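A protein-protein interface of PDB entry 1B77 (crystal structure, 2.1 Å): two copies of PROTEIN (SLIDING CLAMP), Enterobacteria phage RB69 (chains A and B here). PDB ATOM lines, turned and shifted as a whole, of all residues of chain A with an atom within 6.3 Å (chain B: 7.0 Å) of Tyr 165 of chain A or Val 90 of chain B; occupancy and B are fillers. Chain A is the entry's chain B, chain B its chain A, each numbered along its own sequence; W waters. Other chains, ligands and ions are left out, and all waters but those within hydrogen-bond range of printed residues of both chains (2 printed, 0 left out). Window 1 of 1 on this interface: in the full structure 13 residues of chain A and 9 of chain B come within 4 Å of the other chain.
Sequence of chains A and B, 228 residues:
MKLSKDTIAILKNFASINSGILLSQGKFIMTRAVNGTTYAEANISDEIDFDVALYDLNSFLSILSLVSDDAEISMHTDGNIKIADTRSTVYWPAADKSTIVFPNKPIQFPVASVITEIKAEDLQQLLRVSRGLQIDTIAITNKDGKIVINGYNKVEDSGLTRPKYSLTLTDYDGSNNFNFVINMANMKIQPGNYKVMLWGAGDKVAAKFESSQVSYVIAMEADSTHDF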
ATOM      1  N   ASP A 122      22.162 -12.114  -6.901  1.00  0.00           N
ATOM      2  CA  ASP A 122      22.748 -11.913  -8.219  1.00  0.00           C
ATOM      3  C   ASP A 122      23.174 -13.234  -8.861  1.00  0.00           C
ATOM      4  O   ASP A 122      22.980 -13.435 -10.064  1.00  0.00           O
ATOM      5  CB  ASP A 122      23.927 -10.944  -8.104  1.00  0.00           C
ATOM      6  CG  ASP A 122      23.492  -9.563  -7.630  1.00  0.00           C
ATOM      7  OD1 ASP A 122      22.278  -9.275  -7.674  1.00  0.00           O
ATOM      8  OD2 ASP A 122      24.357  -8.758  -7.224  1.00  0.00           O
ATOM      9  N   GLN A 125      20.145 -14.920 -10.207  1.00  0.00           N
ATOM     10  CA  GLN A 125      19.710 -14.384 -11.492  1.00  0.00           C
ATOM     11  C   GLN A 125      20.629 -14.861 -12.625  1.00  0.00           C
ATOM     12  O   GLN A 125      20.152 -15.239 -13.700  1.00  0.00           O
ATOM     13  CB  GLN A 125      19.676 -12.856 -11.464  1.00  0.00           C
ATOM     14  CG  GLN A 125      19.058 -12.246 -12.706  1.00  0.00           C
ATOM     15  CD  GLN A 125      19.151 -10.733 -12.718  1.00  0.00           C
ATOM     16  OE1 GLN A 125      20.219 -10.165 -12.949  1.00  0.00           O
ATOM     17  NE2 GLN A 125      18.031 -10.071 -12.459  1.00  0.00           N
ATOM     18  N   LEU A 126      21.939 -14.841 -12.386  1.00  0.00           N
ATOM     19  CA  LEU A 126      22.902 -15.288 -13.392  1.00  0.00           C
ATOM     20  C   LEU A 126      22.529 -16.687 -13.866  1.00  0.00           C
ATOM     21  O   LEU A 126      22.353 -16.926 -15.063  1.00  0.00           O
ATOM     22  CB  LEU A 126      24.320 -15.329 -12.811  1.00  0.00           C
ATOM     23  CG  LEU A 126      25.411 -15.928 -13.709  1.00  0.00           C
ATOM     24  CD1 LEU A 126      25.521 -15.111 -14.999  1.00  0.00           C
ATOM     25  CD2 LEU A 126      26.749 -15.937 -12.975  1.00  0.00           C
ATOM     26  N   VAL A 129      18.874 -16.756 -15.579  1.00  0.00           N
ATOM     27  CA  VAL A 129      18.881 -16.130 -16.892  1.00  0.00           C
ATOM     28  C   VAL A 129      19.626 -16.951 -17.939  1.00  0.00           C
ATOM     29  O   VAL A 129      19.161 -17.094 -19.072  1.00  0.00           O
ATOM     30  CB  VAL A 129      19.491 -14.719 -16.831  1.00  0.00           C
ATOM     31  CG1 VAL A 129      19.686 -14.184 -18.230  1.00  0.00           C
ATOM     32  CG2 VAL A 129      18.578 -13.785 -16.046  1.00  0.00           C
ATOM     33  N   SER A 130      20.785 -17.487 -17.564  1.00  0.00           N
ATOM     34  CA  SER A 130      21.589 -18.289 -18.480  1.00  0.00           C
ATOM     35  C   SER A 130      20.737 -19.352 -19.164  1.00  0.00           C
ATOM     36  O   SER A 130      20.813 -19.537 -20.378  1.00  0.00           O
ATOM     37  CB  SER A 130      22.738 -18.955 -17.721  1.00  0.00           C
ATOM     38  OG  SER A 130      23.545 -17.975 -17.092  1.00  0.00           O
ATOM     39  N   LEU A 133      18.242 -17.774 -21.712  1.00  0.00           N
ATOM     40  CA  LEU A 133      18.882 -17.125 -22.856  1.00  0.00           C
ATOM     41  C   LEU A 133      19.868 -18.013 -23.606  1.00  0.00           C
ATOM     42  O   LEU A 133      20.535 -17.552 -24.534  1.00  0.00           O
ATOM     43  CB  LEU A 133      19.637 -15.874 -22.404  1.00  0.00           C
ATOM     44  CG  LEU A 133      18.913 -14.655 -21.839  1.00  0.00           C
ATOM     45  CD1 LEU A 133      19.963 -13.696 -21.290  1.00  0.00           C
ATOM     46  CD2 LEU A 133      18.079 -13.977 -22.914  1.00  0.00           C
ATOM     47  N   ILE A 135      22.730 -19.262 -22.515  1.00  0.00           N
ATOM     48  CA  ILE A 135      24.075 -18.743 -22.269  1.00  0.00           C
ATOM     49  C   ILE A 135      24.952 -19.929 -21.870  1.00  0.00           C
ATOM     50  O   ILE A 135      24.710 -20.574 -20.846  1.00  0.00           O
ATOM     51  CB  ILE A 135      24.077 -17.708 -21.124  1.00  0.00           C
ATOM     52  CG1 ILE A 135      23.335 -16.444 -21.564  1.00  0.00           C
ATOM     53  CG2 ILE A 135      25.506 -17.378 -20.722  1.00  0.00           C
ATOM     54  CD1 ILE A 135      23.136 -15.447 -20.446  1.00  0.00           C
ATOM     55  N   ILE A 138      30.415 -17.410 -19.877  1.00  0.00           N
ATOM     56  CA  ILE A 138      30.453 -16.109 -19.217  1.00  0.00           C
ATOM     57  C   ILE A 138      31.885 -15.605 -19.163  1.00  0.00           C
ATOM     58  O   ILE A 138      32.840 -16.385 -19.169  1.00  0.00           O
ATOM     59  CB  ILE A 138      29.925 -16.127 -17.754  1.00  0.00           C
ATOM     60  CG1 ILE A 138      30.628 -17.230 -16.953  1.00  0.00           C
ATOM     61  CG2 ILE A 138      28.406 -16.232 -17.749  1.00  0.00           C
ATOM     62  CD1 ILE A 138      30.415 -17.143 -15.447  1.00  0.00           C
ATOM     63  N   ILE A 149      30.237  -9.377 -15.265  1.00  0.00           N
ATOM     64  CA  ILE A 149      30.124 -10.671 -15.912  1.00  0.00           C
ATOM     65  C   ILE A 149      29.217 -10.505 -17.127  1.00  0.00           C
ATOM     66  O   ILE A 149      28.117  -9.963 -17.011  1.00  0.00           O
ATOM     67  CB  ILE A 149      29.465 -11.729 -14.994  1.00  0.00           C
ATOM     68  CG1 ILE A 149      30.293 -11.931 -13.726  1.00  0.00           C
ATOM     69  CG2 ILE A 149      29.344 -13.056 -15.742  1.00  0.00           C
ATOM     70  CD1 ILE A 149      29.610 -12.842 -12.693  1.00  0.00           C
ATOM     71  N   ASN A 150      29.700 -10.949 -18.282  1.00  0.00           N
ATOM     72  CA  ASN A 150      28.938 -10.911 -19.521  1.00  0.00           C
ATOM     73  C   ASN A 150      28.636 -12.353 -19.929  1.00  0.00           C
ATOM     74  O   ASN A 150      29.522 -13.210 -19.886  1.00  0.00           O
ATOM     75  CB  ASN A 150      29.735 -10.228 -20.638  1.00  0.00           C
ATOM     76  CG  ASN A 150      29.981  -8.766 -20.362  1.00  0.00           C
ATOM     77  OD1 ASN A 150      29.048  -8.011 -20.106  1.00  0.00           O
ATOM     78  ND2 ASN A 150      31.244  -8.358 -20.411  1.00  0.00           N
ATOM     79  N   GLY A 151      27.394 -12.616 -20.315  1.00  0.00           N
ATOM     80  CA  GLY A 151      27.015 -13.954 -20.731  1.00  0.00           C
ATOM     81  C   GLY A 151      26.916 -14.049 -22.245  1.00  0.00           C
ATOM     82  O   GLY A 151      26.374 -13.151 -22.893  1.00  0.00           O
ATOM     83  N   TYR A 152      27.447 -15.125 -22.821  1.00  0.00           N
ATOM     84  CA  TYR A 152      27.397 -15.298 -24.271  1.00  0.00           C
ATOM     85  C   TYR A 152      26.918 -16.679 -24.688  1.00  0.00           C
ATOM     86  O   TYR A 152      26.844 -17.602 -23.877  1.00  0.00           O
ATOM     87  CB  TYR A 152      28.780 -15.096 -24.902  1.00  0.00           C
ATOM     88  CG  TYR A 152      29.491 -13.819 -24.528  1.00  0.00           C
ATOM     89  CD1 TYR A 152      30.188 -13.715 -23.324  1.00  0.00           C
ATOM     90  CD2 TYR A 152      29.486 -12.722 -25.384  1.00  0.00           C
ATOM     91  CE1 TYR A 152      30.867 -12.552 -22.983  1.00  0.00           C
ATOM     92  CE2 TYR A 152      30.158 -11.555 -25.056  1.00  0.00           C
ATOM     93  CZ  TYR A 152      30.848 -11.474 -23.854  1.00  0.00           C
ATOM     94  OH  TYR A 152      31.513 -10.320 -23.520  1.00  0.00           O
ATOM     95  N   ARG A 162      28.987 -10.534 -28.625  1.00  0.00           N
ATOM     96  CA  ARG A 162      27.631 -10.028 -28.481  1.00  0.00           C
ATOM     97  C   ARG A 162      26.952 -10.506 -27.204  1.00  0.00           C
ATOM     98  O   ARG A 162      26.167 -11.442 -27.232  1.00  0.00           O
ATOM     99  CB  ARG A 162      26.802 -10.436 -29.702  1.00  0.00           C
ATOM    100  CG  ARG A 162      27.369  -9.921 -31.021  1.00  0.00           C
ATOM    101  CD  ARG A 162      26.542 -10.378 -32.211  1.00  0.00           C
ATOM    102  NE  ARG A 162      26.663 -11.813 -32.462  1.00  0.00           N
ATOM    103  CZ  ARG A 162      27.697 -12.387 -33.072  1.00  0.00           C
ATOM    104  NH1 ARG A 162      28.714 -11.648 -33.506  1.00  0.00           N
ATOM    105  NH2 ARG A 162      27.717 -13.703 -33.249  1.00  0.00           N
ATOM    106  N   PRO A 163      27.242  -9.852 -26.070  1.00  0.00           N
ATOM    107  CA  PRO A 163      26.663 -10.206 -24.772  1.00  0.00           C
ATOM    108  C   PRO A 163      25.138 -10.197 -24.719  1.00  0.00           C
ATOM    109  O   PRO A 163      24.491  -9.255 -25.187  1.00  0.00           O
ATOM    110  CB  PRO A 163      27.281  -9.175 -23.835  1.00  0.00           C
ATOM    111  CG  PRO A 163      27.530  -8.008 -24.727  1.00  0.00           C
ATOM    112  CD  PRO A 163      28.108  -8.670 -25.936  1.00  0.00           C
ATOM    113  N   LYS A 164      24.577 -11.249 -24.131  1.00  0.00           N
ATOM    114  CA  LYS A 164      23.127 -11.400 -24.008  1.00  0.00           C
ATOM    115  C   LYS A 164      22.683 -11.050 -22.586  1.00  0.00           C
ATOM    116  O   LYS A 164      21.489 -10.932 -22.296  1.00  0.00           O
ATOM    117  CB  LYS A 164      22.737 -12.842 -24.349  1.00  0.00           C
ATOM    118  CG  LYS A 164      23.342 -13.320 -25.666  1.00  0.00           C
ATOM    119  CD  LYS A 164      23.014 -14.763 -25.989  1.00  0.00           C
ATOM    120  CE  LYS A 164      21.609 -14.921 -26.531  1.00  0.00           C
ATOM    121  NZ  LYS A 164      21.337 -16.346 -26.893  1.00  0.00           N
ATOM    122  N   TYR A 165      23.665 -10.882 -21.711  1.00  0.00           N
ATOM    123  CA  TYR A 165      23.424 -10.547 -20.320  1.00  0.00           C
ATOM    124  C   TYR A 165      24.674  -9.885 -19.768  1.00  0.00           C
ATOM    125  O   TYR A 165      25.795 -10.139 -20.234  1.00  0.00           O
ATOM    126  CB  TYR A 165      23.123 -11.812 -19.517  1.00  0.00           C
ATOM    127  CG  TYR A 165      22.988 -11.616 -18.021  1.00  0.00           C
ATOM    128  CD1 TYR A 165      21.896 -10.948 -17.475  1.00  0.00           C
ATOM    129  CD2 TYR A 165      23.928 -12.159 -17.148  1.00  0.00           C
ATOM    130  CE1 TYR A 165      21.735 -10.836 -16.088  1.00  0.00           C
ATOM    131  CE2 TYR A 165      23.781 -12.051 -15.769  1.00  0.00           C
ATOM    132  CZ  TYR A 165      22.681 -11.394 -15.243  1.00  0.00           C
ATOM    133  OH  TYR A 165      22.529 -11.318 -13.875  1.00  0.00           O
ATOM    134  N   SER A 166      24.474  -9.036 -18.769  1.00  0.00           N
ATOM    135  CA  SER A 166      25.572  -8.343 -18.129  1.00  0.00           C
ATOM    136  C   SER A 166      25.194  -8.049 -16.685  1.00  0.00           C
ATOM    137  O   SER A 166      24.112  -7.526 -16.412  1.00  0.00           O
ATOM    138  CB  SER A 166      25.873  -7.046 -18.873  1.00  0.00           C
ATOM    139  OG  SER A 166      27.067  -6.475 -18.380  1.00  0.00           O
ATOM    140  N   LEU A 167      26.082  -8.404 -15.762  1.00  0.00           N
ATOM    141  CA  LEU A 167      25.851  -8.186 -14.341  1.00  0.00           C
ATOM    142  C   LEU A 167      27.049  -7.459 -13.758  1.00  0.00           C
ATOM    143  O   LEU A 167      28.193  -7.855 -13.982  1.00  0.00           O
ATOM    144  CB  LEU A 167      25.660  -9.520 -13.617  1.00  0.00           C
ATOM    145  CG  LEU A 167      25.655  -9.490 -12.079  1.00  0.00           C
ATOM    146  CD1 LEU A 167      24.327  -8.937 -11.565  1.00  0.00           C
ATOM    147  CD2 LEU A 167      25.887 -10.893 -11.548  1.00  0.00           C
ATOM    148  N   ILE B  63      11.567 -14.680 -19.006  1.00  0.00           N
ATOM    149  CA  ILE B  63      12.753 -13.916 -18.653  1.00  0.00           C
ATOM    150  C   ILE B  63      12.408 -12.705 -17.771  1.00  0.00           C
ATOM    151  O   ILE B  63      13.197 -12.309 -16.910  1.00  0.00           O
ATOM    152  CB  ILE B  63      13.500 -13.469 -19.936  1.00  0.00           C
ATOM    153  CG1 ILE B  63      14.612 -14.475 -20.244  1.00  0.00           C
ATOM    154  CG2 ILE B  63      14.051 -12.058 -19.794  1.00  0.00           C
ATOM    155  CD1 ILE B  63      15.658 -14.570 -19.162  1.00  0.00           C
ATOM    156  N   LEU B  66      12.461 -13.056 -13.990  1.00  0.00           N
ATOM    157  CA  LEU B  66      13.761 -13.095 -13.319  1.00  0.00           C
ATOM    158  C   LEU B  66      14.348 -11.734 -12.963  1.00  0.00           C
ATOM    159  O   LEU B  66      15.417 -11.666 -12.362  1.00  0.00           O
ATOM    160  CB  LEU B  66      14.772 -13.862 -14.179  1.00  0.00           C
ATOM    161  CG  LEU B  66      14.423 -15.319 -14.498  1.00  0.00           C
ATOM    162  CD1 LEU B  66      15.493 -15.925 -15.392  1.00  0.00           C
ATOM    163  CD2 LEU B  66      14.287 -16.111 -13.199  1.00  0.00           C
ATOM    164  N   VAL B  67      13.668 -10.653 -13.340  1.00  0.00           N
ATOM    165  CA  VAL B  67      14.156  -9.304 -13.038  1.00  0.00           C
ATOM    166  C   VAL B  67      13.146  -8.502 -12.214  1.00  0.00           C
ATOM    167  O   VAL B  67      12.023  -8.951 -11.990  1.00  0.00           O
ATOM    168  CB  VAL B  67      14.475  -8.521 -14.332  1.00  0.00           C
ATOM    169  CG1 VAL B  67      15.605  -9.202 -15.084  1.00  0.00           C
ATOM    170  CG2 VAL B  67      13.228  -8.435 -15.216  1.00  0.00           C
ATOM    171  N   ILE B  81      16.112  -5.816 -28.090  1.00  0.00           N
ATOM    172  CA  ILE B  81      15.461  -5.343 -26.881  1.00  0.00           C
ATOM    173  C   ILE B  81      16.368  -5.338 -25.669  1.00  0.00           C
ATOM    174  O   ILE B  81      17.120  -6.291 -25.443  1.00  0.00           O
ATOM    175  CB  ILE B  81      14.260  -6.221 -26.520  1.00  0.00           C
ATOM    176  CG1 ILE B  81      13.283  -6.275 -27.686  1.00  0.00           C
ATOM    177  CG2 ILE B  81      13.602  -5.696 -25.260  1.00  0.00           C
ATOM    178  CD1 ILE B  81      12.279  -7.388 -27.550  1.00  0.00           C
ATOM    179  N   LYS B  82      16.273  -4.272 -24.879  1.00  0.00           N
ATOM    180  CA  LYS B  82      17.048  -4.143 -23.657  1.00  0.00           C
ATOM    181  C   LYS B  82      16.137  -4.138 -22.434  1.00  0.00           C
ATOM    182  O   LYS B  82      15.139  -3.426 -22.395  1.00  0.00           O
ATOM    183  CB  LYS B  82      17.882  -2.857 -23.661  1.00  0.00           C
ATOM    184  CG  LYS B  82      18.585  -2.621 -22.327  1.00  0.00           C
ATOM    185  CD  LYS B  82      19.365  -1.316 -22.282  1.00  0.00           C
ATOM    186  CE  LYS B  82      19.921  -1.072 -20.871  1.00  0.00           C
ATOM    187  NZ  LYS B  82      20.870   0.086 -20.816  1.00  0.00           N
ATOM    188  N   ILE B  83      16.494  -4.937 -21.436  1.00  0.00           N
ATOM    189  CA  ILE B  83      15.728  -5.018 -20.202  1.00  0.00           C
ATOM    190  C   ILE B  83      16.638  -4.541 -19.076  1.00  0.00           C
ATOM    191  O   ILE B  83      17.558  -5.254 -18.655  1.00  0.00           O
ATOM    192  CB  ILE B  83      15.276  -6.461 -19.921  1.00  0.00           C
ATOM    193  CG1 ILE B  83      14.510  -7.004 -21.133  1.00  0.00           C
ATOM    194  CG2 ILE B  83      14.401  -6.499 -18.676  1.00  0.00           C
ATOM    195  CD1 ILE B  83      14.259  -8.496 -21.086  1.00  0.00           C
ATOM    196  N   ALA B  84      16.378  -3.326 -18.599  1.00  0.00           N
ATOM    197  CA  ALA B  84      17.184  -2.716 -17.547  1.00  0.00           C
ATOM    198  C   ALA B  84      16.728  -3.056 -16.135  1.00  0.00           C
ATOM    199  O   ALA B  84      15.636  -2.673 -15.716  1.00  0.00           O
ATOM    200  CB  ALA B  84      17.212  -1.197 -17.735  1.00  0.00           C
ATOM    201  N   ASP B  85      17.580  -3.772 -15.406  1.00  0.00           N
ATOM    202  CA  ASP B  85      17.285  -4.166 -14.026  1.00  0.00           C
ATOM    203  C   ASP B  85      18.216  -3.385 -13.083  1.00  0.00           C
ATOM    204  O   ASP B  85      19.067  -2.627 -13.545  1.00  0.00           O
ATOM    205  CB  ASP B  85      17.482  -5.677 -13.869  1.00  0.00           C
ATOM    206  CG  ASP B  85      16.865  -6.220 -12.598  1.00  0.00           C
ATOM    207  OD1 ASP B  85      16.028  -5.523 -11.988  1.00  0.00           O
ATOM    208  OD2 ASP B  85      17.201  -7.361 -12.219  1.00  0.00           O
ATOM    209  N   ARG B  87      21.027  -4.002 -11.035  1.00  0.00           N
ATOM    210  CA  ARG B  87      22.468  -4.083 -11.296  1.00  0.00           C
ATOM    211  C   ARG B  87      22.809  -4.884 -12.548  1.00  0.00           C
ATOM    212  O   ARG B  87      23.976  -5.175 -12.797  1.00  0.00           O
ATOM    213  CB  ARG B  87      23.212  -4.750 -10.138  1.00  0.00           C
ATOM    214  CG  ARG B  87      22.756  -4.397  -8.752  1.00  0.00           C
ATOM    215  CD  ARG B  87      22.000  -5.572  -8.166  1.00  0.00           C
ATOM    216  NE  ARG B  87      21.982  -5.554  -6.707  1.00  0.00           N
ATOM    217  CZ  ARG B  87      21.322  -6.437  -5.961  1.00  0.00           C
ATOM    218  NH1 ARG B  87      20.624  -7.405  -6.545  1.00  0.00           N
ATOM    219  NH2 ARG B  87      21.361  -6.354  -4.632  1.00  0.00           N
ATOM    220  N   SER B  88      21.808  -5.259 -13.327  1.00  0.00           N
ATOM    221  CA  SER B  88      22.072  -6.054 -14.513  1.00  0.00           C
ATOM    222  C   SER B  88      21.234  -5.623 -15.695  1.00  0.00           C
ATOM    223  O   SER B  88      20.327  -4.794 -15.565  1.00  0.00           O
ATOM    224  CB  SER B  88      21.812  -7.530 -14.212  1.00  0.00           C
ATOM    225  OG  SER B  88      20.496  -7.704 -13.717  1.00  0.00           O
ATOM    226  N   THR B  89      21.542  -6.205 -16.848  1.00  0.00           N
ATOM    227  CA  THR B  89      20.838  -5.906 -18.086  1.00  0.00           C
ATOM    228  C   THR B  89      20.631  -7.210 -18.867  1.00  0.00           C
ATOM    229  O   THR B  89      21.517  -8.065 -18.924  1.00  0.00           O
ATOM    230  CB  THR B  89      21.661  -4.920 -18.955  1.00  0.00           C
ATOM    231  OG1 THR B  89      21.924  -3.732 -18.205  1.00  0.00           O
ATOM    232  CG2 THR B  89      20.911  -4.551 -20.226  1.00  0.00           C
ATOM    233  N   VAL B  90      19.452  -7.368 -19.450  1.00  0.00           N
ATOM    234  CA  VAL B  90      19.160  -8.548 -20.244  1.00  0.00           C
ATOM    235  C   VAL B  90      18.816  -8.087 -21.648  1.00  0.00           C
ATOM    236  O   VAL B  90      17.962  -7.223 -21.828  1.00  0.00           O
ATOM    237  CB  VAL B  90      17.946  -9.346 -19.693  1.00  0.00           C
ATOM    238  CG1 VAL B  90      17.608 -10.494 -20.649  1.00  0.00           C
ATOM    239  CG2 VAL B  90      18.246  -9.883 -18.300  1.00  0.00           C
ATOM    240  N   TYR B  91      19.484  -8.655 -22.646  1.00  0.00           N
ATOM    241  CA  TYR B  91      19.191  -8.305 -24.025  1.00  0.00           C
ATOM    242  C   TYR B  91      18.406  -9.456 -24.637  1.00  0.00           C
ATOM    243  O   TYR B  91      18.724 -10.621 -24.403  1.00  0.00           O
ATOM    244  CB  TYR B  91      20.479  -8.060 -24.812  1.00  0.00           C
ATOM    245  CG  TYR B  91      21.323  -6.949 -24.239  1.00  0.00           C
ATOM    246  CD1 TYR B  91      20.966  -5.613 -24.412  1.00  0.00           C
ATOM    247  CD2 TYR B  91      22.473  -7.235 -23.510  1.00  0.00           C
ATOM    248  CE1 TYR B  91      21.736  -4.584 -23.871  1.00  0.00           C
ATOM    249  CE2 TYR B  91      23.250  -6.217 -22.967  1.00  0.00           C
ATOM    250  CZ  TYR B  91      22.879  -4.897 -23.148  1.00  0.00           C
ATOM    251  OH  TYR B  91      23.651  -3.902 -22.596  1.00  0.00           O
ATOM    252  N   TRP B  92      17.368  -9.126 -25.402  1.00  0.00           N
ATOM    253  CA  TRP B  92      16.539 -10.138 -26.046  1.00  0.00           C
ATOM    254  C   TRP B  92      16.414  -9.798 -27.529  1.00  0.00           C
ATOM    255  O   TRP B  92      16.220  -8.645 -27.900  1.00  0.00           O
ATOM    256  CB  TRP B  92      15.155 -10.191 -25.380  1.00  0.00           C
ATOM    257  CG  TRP B  92      14.336 -11.387 -25.785  1.00  0.00           C
ATOM    258  CD1 TRP B  92      13.501 -11.487 -26.864  1.00  0.00           C
ATOM    259  CD2 TRP B  92      14.303 -12.665 -25.135  1.00  0.00           C
ATOM    260  NE1 TRP B  92      12.953 -12.744 -26.924  1.00  0.00           N
ATOM    261  CE2 TRP B  92      13.430 -13.488 -25.877  1.00  0.00           C
ATOM    262  CE3 TRP B  92      14.936 -13.192 -23.998  1.00  0.00           C
ATOM    263  CZ2 TRP B  92      13.160 -14.814 -25.517  1.00  0.00           C
ATOM    264  CZ3 TRP B  92      14.672 -14.520 -23.641  1.00  0.00           C
ATOM    265  CH2 TRP B  92      13.792 -15.312 -24.403  1.00  0.00           C
HETATM  266  O   HOH W   1      16.343  -8.483  -9.899  1.00  0.00           O
HETATM  267  O   HOH W   2      24.024  -4.131 -16.653  1.00  0.00           O
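No position is printed for both chains.
Of the 18 pairs that touch across the chains among the printed residues, none has its exchanged pair printed and touching as well.
Among the printed residues, merely in contact across the chains: Gln 125 of chain A with Val 67 of chain B (3.7 Å), Val 129 of chain A with Leu 66 of chain B (3.5 Å), Leu 133 of chain A with Tyr 91 of chain B (3.7 Å), Leu 133 of chain A with Trp 92 of chain B (3.4 Å), Pro 163 of chain A with Tyr 91 of chain B (3.3 Å), Lys 164 of chain A with Val 90 of chain B (3.9 Å), Tyr 165 of chain A with Ser 88 of chain B (3.8 Å), Tyr 165 of chain A with Thr 89 of chain B (3.2 Å), Tyr 165 of chain A with Val 90 of chain B (3.9 Å), Ser 166 of chain A with Ser 88 of chain B (3.2 Å), Leu 167 of chain A with Arg 87 of chain B (3.9 Å) and Leu 167 of chain A with Ser 88 of chain B (3.9 Å).
Printed residues of chain A that touch a printed residue of chain B: Asp 122, Gln 125, Val 129, Leu 133, Pro 163, Lys 164, Tyr 165, Ser 166 and Leu 167.
Of the 14 printed residues of chain B, 9 touch a printed residue of chain A.
Printed residues of chain B that touch a printed residue of chain A: Leu 66, Val 67, Asp 85, Arg 87, Ser 88, Thr 89, Val 90, Tyr 91 and Trp 92.
Hydrophobic or aromatic side chains of chain B within 4 Å of the printed part of chain A: Leu 66, Val 67, Val 90, Tyr 91 and Trp 92.
Among the printed residues, Asp or Glu carboxylates within 4 Å of a Lys or Arg side-chain nitrogen of the other chain: Asp 122 of chain A with Arg 87 of chain B (2.7 Å).
Tyr 165 of chain A touches just these residues of chain B: Ser 88, Thr 89 and Val 90.
Val 90 of chain B touches just these residues of chain A: Lys 164 and Tyr 165.
Printed residues of chain B within 4 Å of Gln 125 of chain A: Leu 66, Val 67, Asp 85 and Ser 88.
Of the printed residues of chain A, Ser 88 of chain B touches Gln 125 (2.6 Å), Tyr 165 (3.8 Å), Ser 166 (3.2 Å) and Leu 167 (3.9 Å).
Ile 81 of chain B touches none of the printed residues of chain A.
Ile 138 of chain A touches none of the printed residues of chain B.
The nearest residue of chain A that does not touch Val 90 of chain B is Leu 133 of chain A (4.03 Å).
Water W2 bridges OG1 of Thr 89 of chain B (2.6 Å) and O of Ser 166 of chain A (3.4 Å).
Water W1 bridges the side-chain carboxylate of Asp 85 of chain B (2.7 Å) and the side-chain amide nitrogen of Gln 125 of chain A (3.5 Å).
The backbone NH (N) of Ile 83 of chain B lies within hydrogen-bond range of the backbone carbonyl oxygen (O) of Val 90 of chain B, 2.7 Å away.
OD1 of Asn 150 of chain A is in hydrogen-bond range of OG of Ser 166 of chain A, at 3.0 Å.
The side-chain amide oxygen (OE1) of Gln 125 of chain A is in hydrogen-bond range of the side-chain hydroxyl (OH) of Tyr 165 of chain A (2.7 Å).
The backbone NH of Leu 167 of chain A lies within hydrogen-bond range of the backbone carbonyl oxygen of Ile 149 of chain A, at 2.9 Å.
N of Lys 164 of chain A lies within hydrogen-bond range of O of Gly 151 of chain A.
N of Ile 81 of chain B is in hydrogen-bond range of O of Trp 92 of chain B (2.8 Å).
NH1 of Arg 87 of chain B lies within salt-bridge range of OD1 of Asp 122 of chain A (2.7 Å).
OD2 of Asp 85 of chain B sits at hydrogen-bond distance from NE2 of Gln 125 of chain A.
The backbone NH (N) of Thr 89 of chain B sits at hydrogen-bond distance from the backbone carbonyl oxygen (O) of Ser 166 of chain A (2.9 Å).
The backbone carbonyl oxygen (O) of Lys 164 of chain A lies within hydrogen-bond range of the backbone NH (N) of Tyr 91 of chain B (3.1 Å).
The side-chain amide oxygen (OE1) of Gln 125 of chain A is in hydrogen-bond range of the side-chain hydroxyl (OG) of Ser 88 of chain B (2.6 Å).
The backbone carbonyl oxygen (O) of Leu 66 of chain B lies within hydrogen-bond range of the side-chain amide nitrogen (NE2) of Gln 125 of chain A (3.1 Å).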
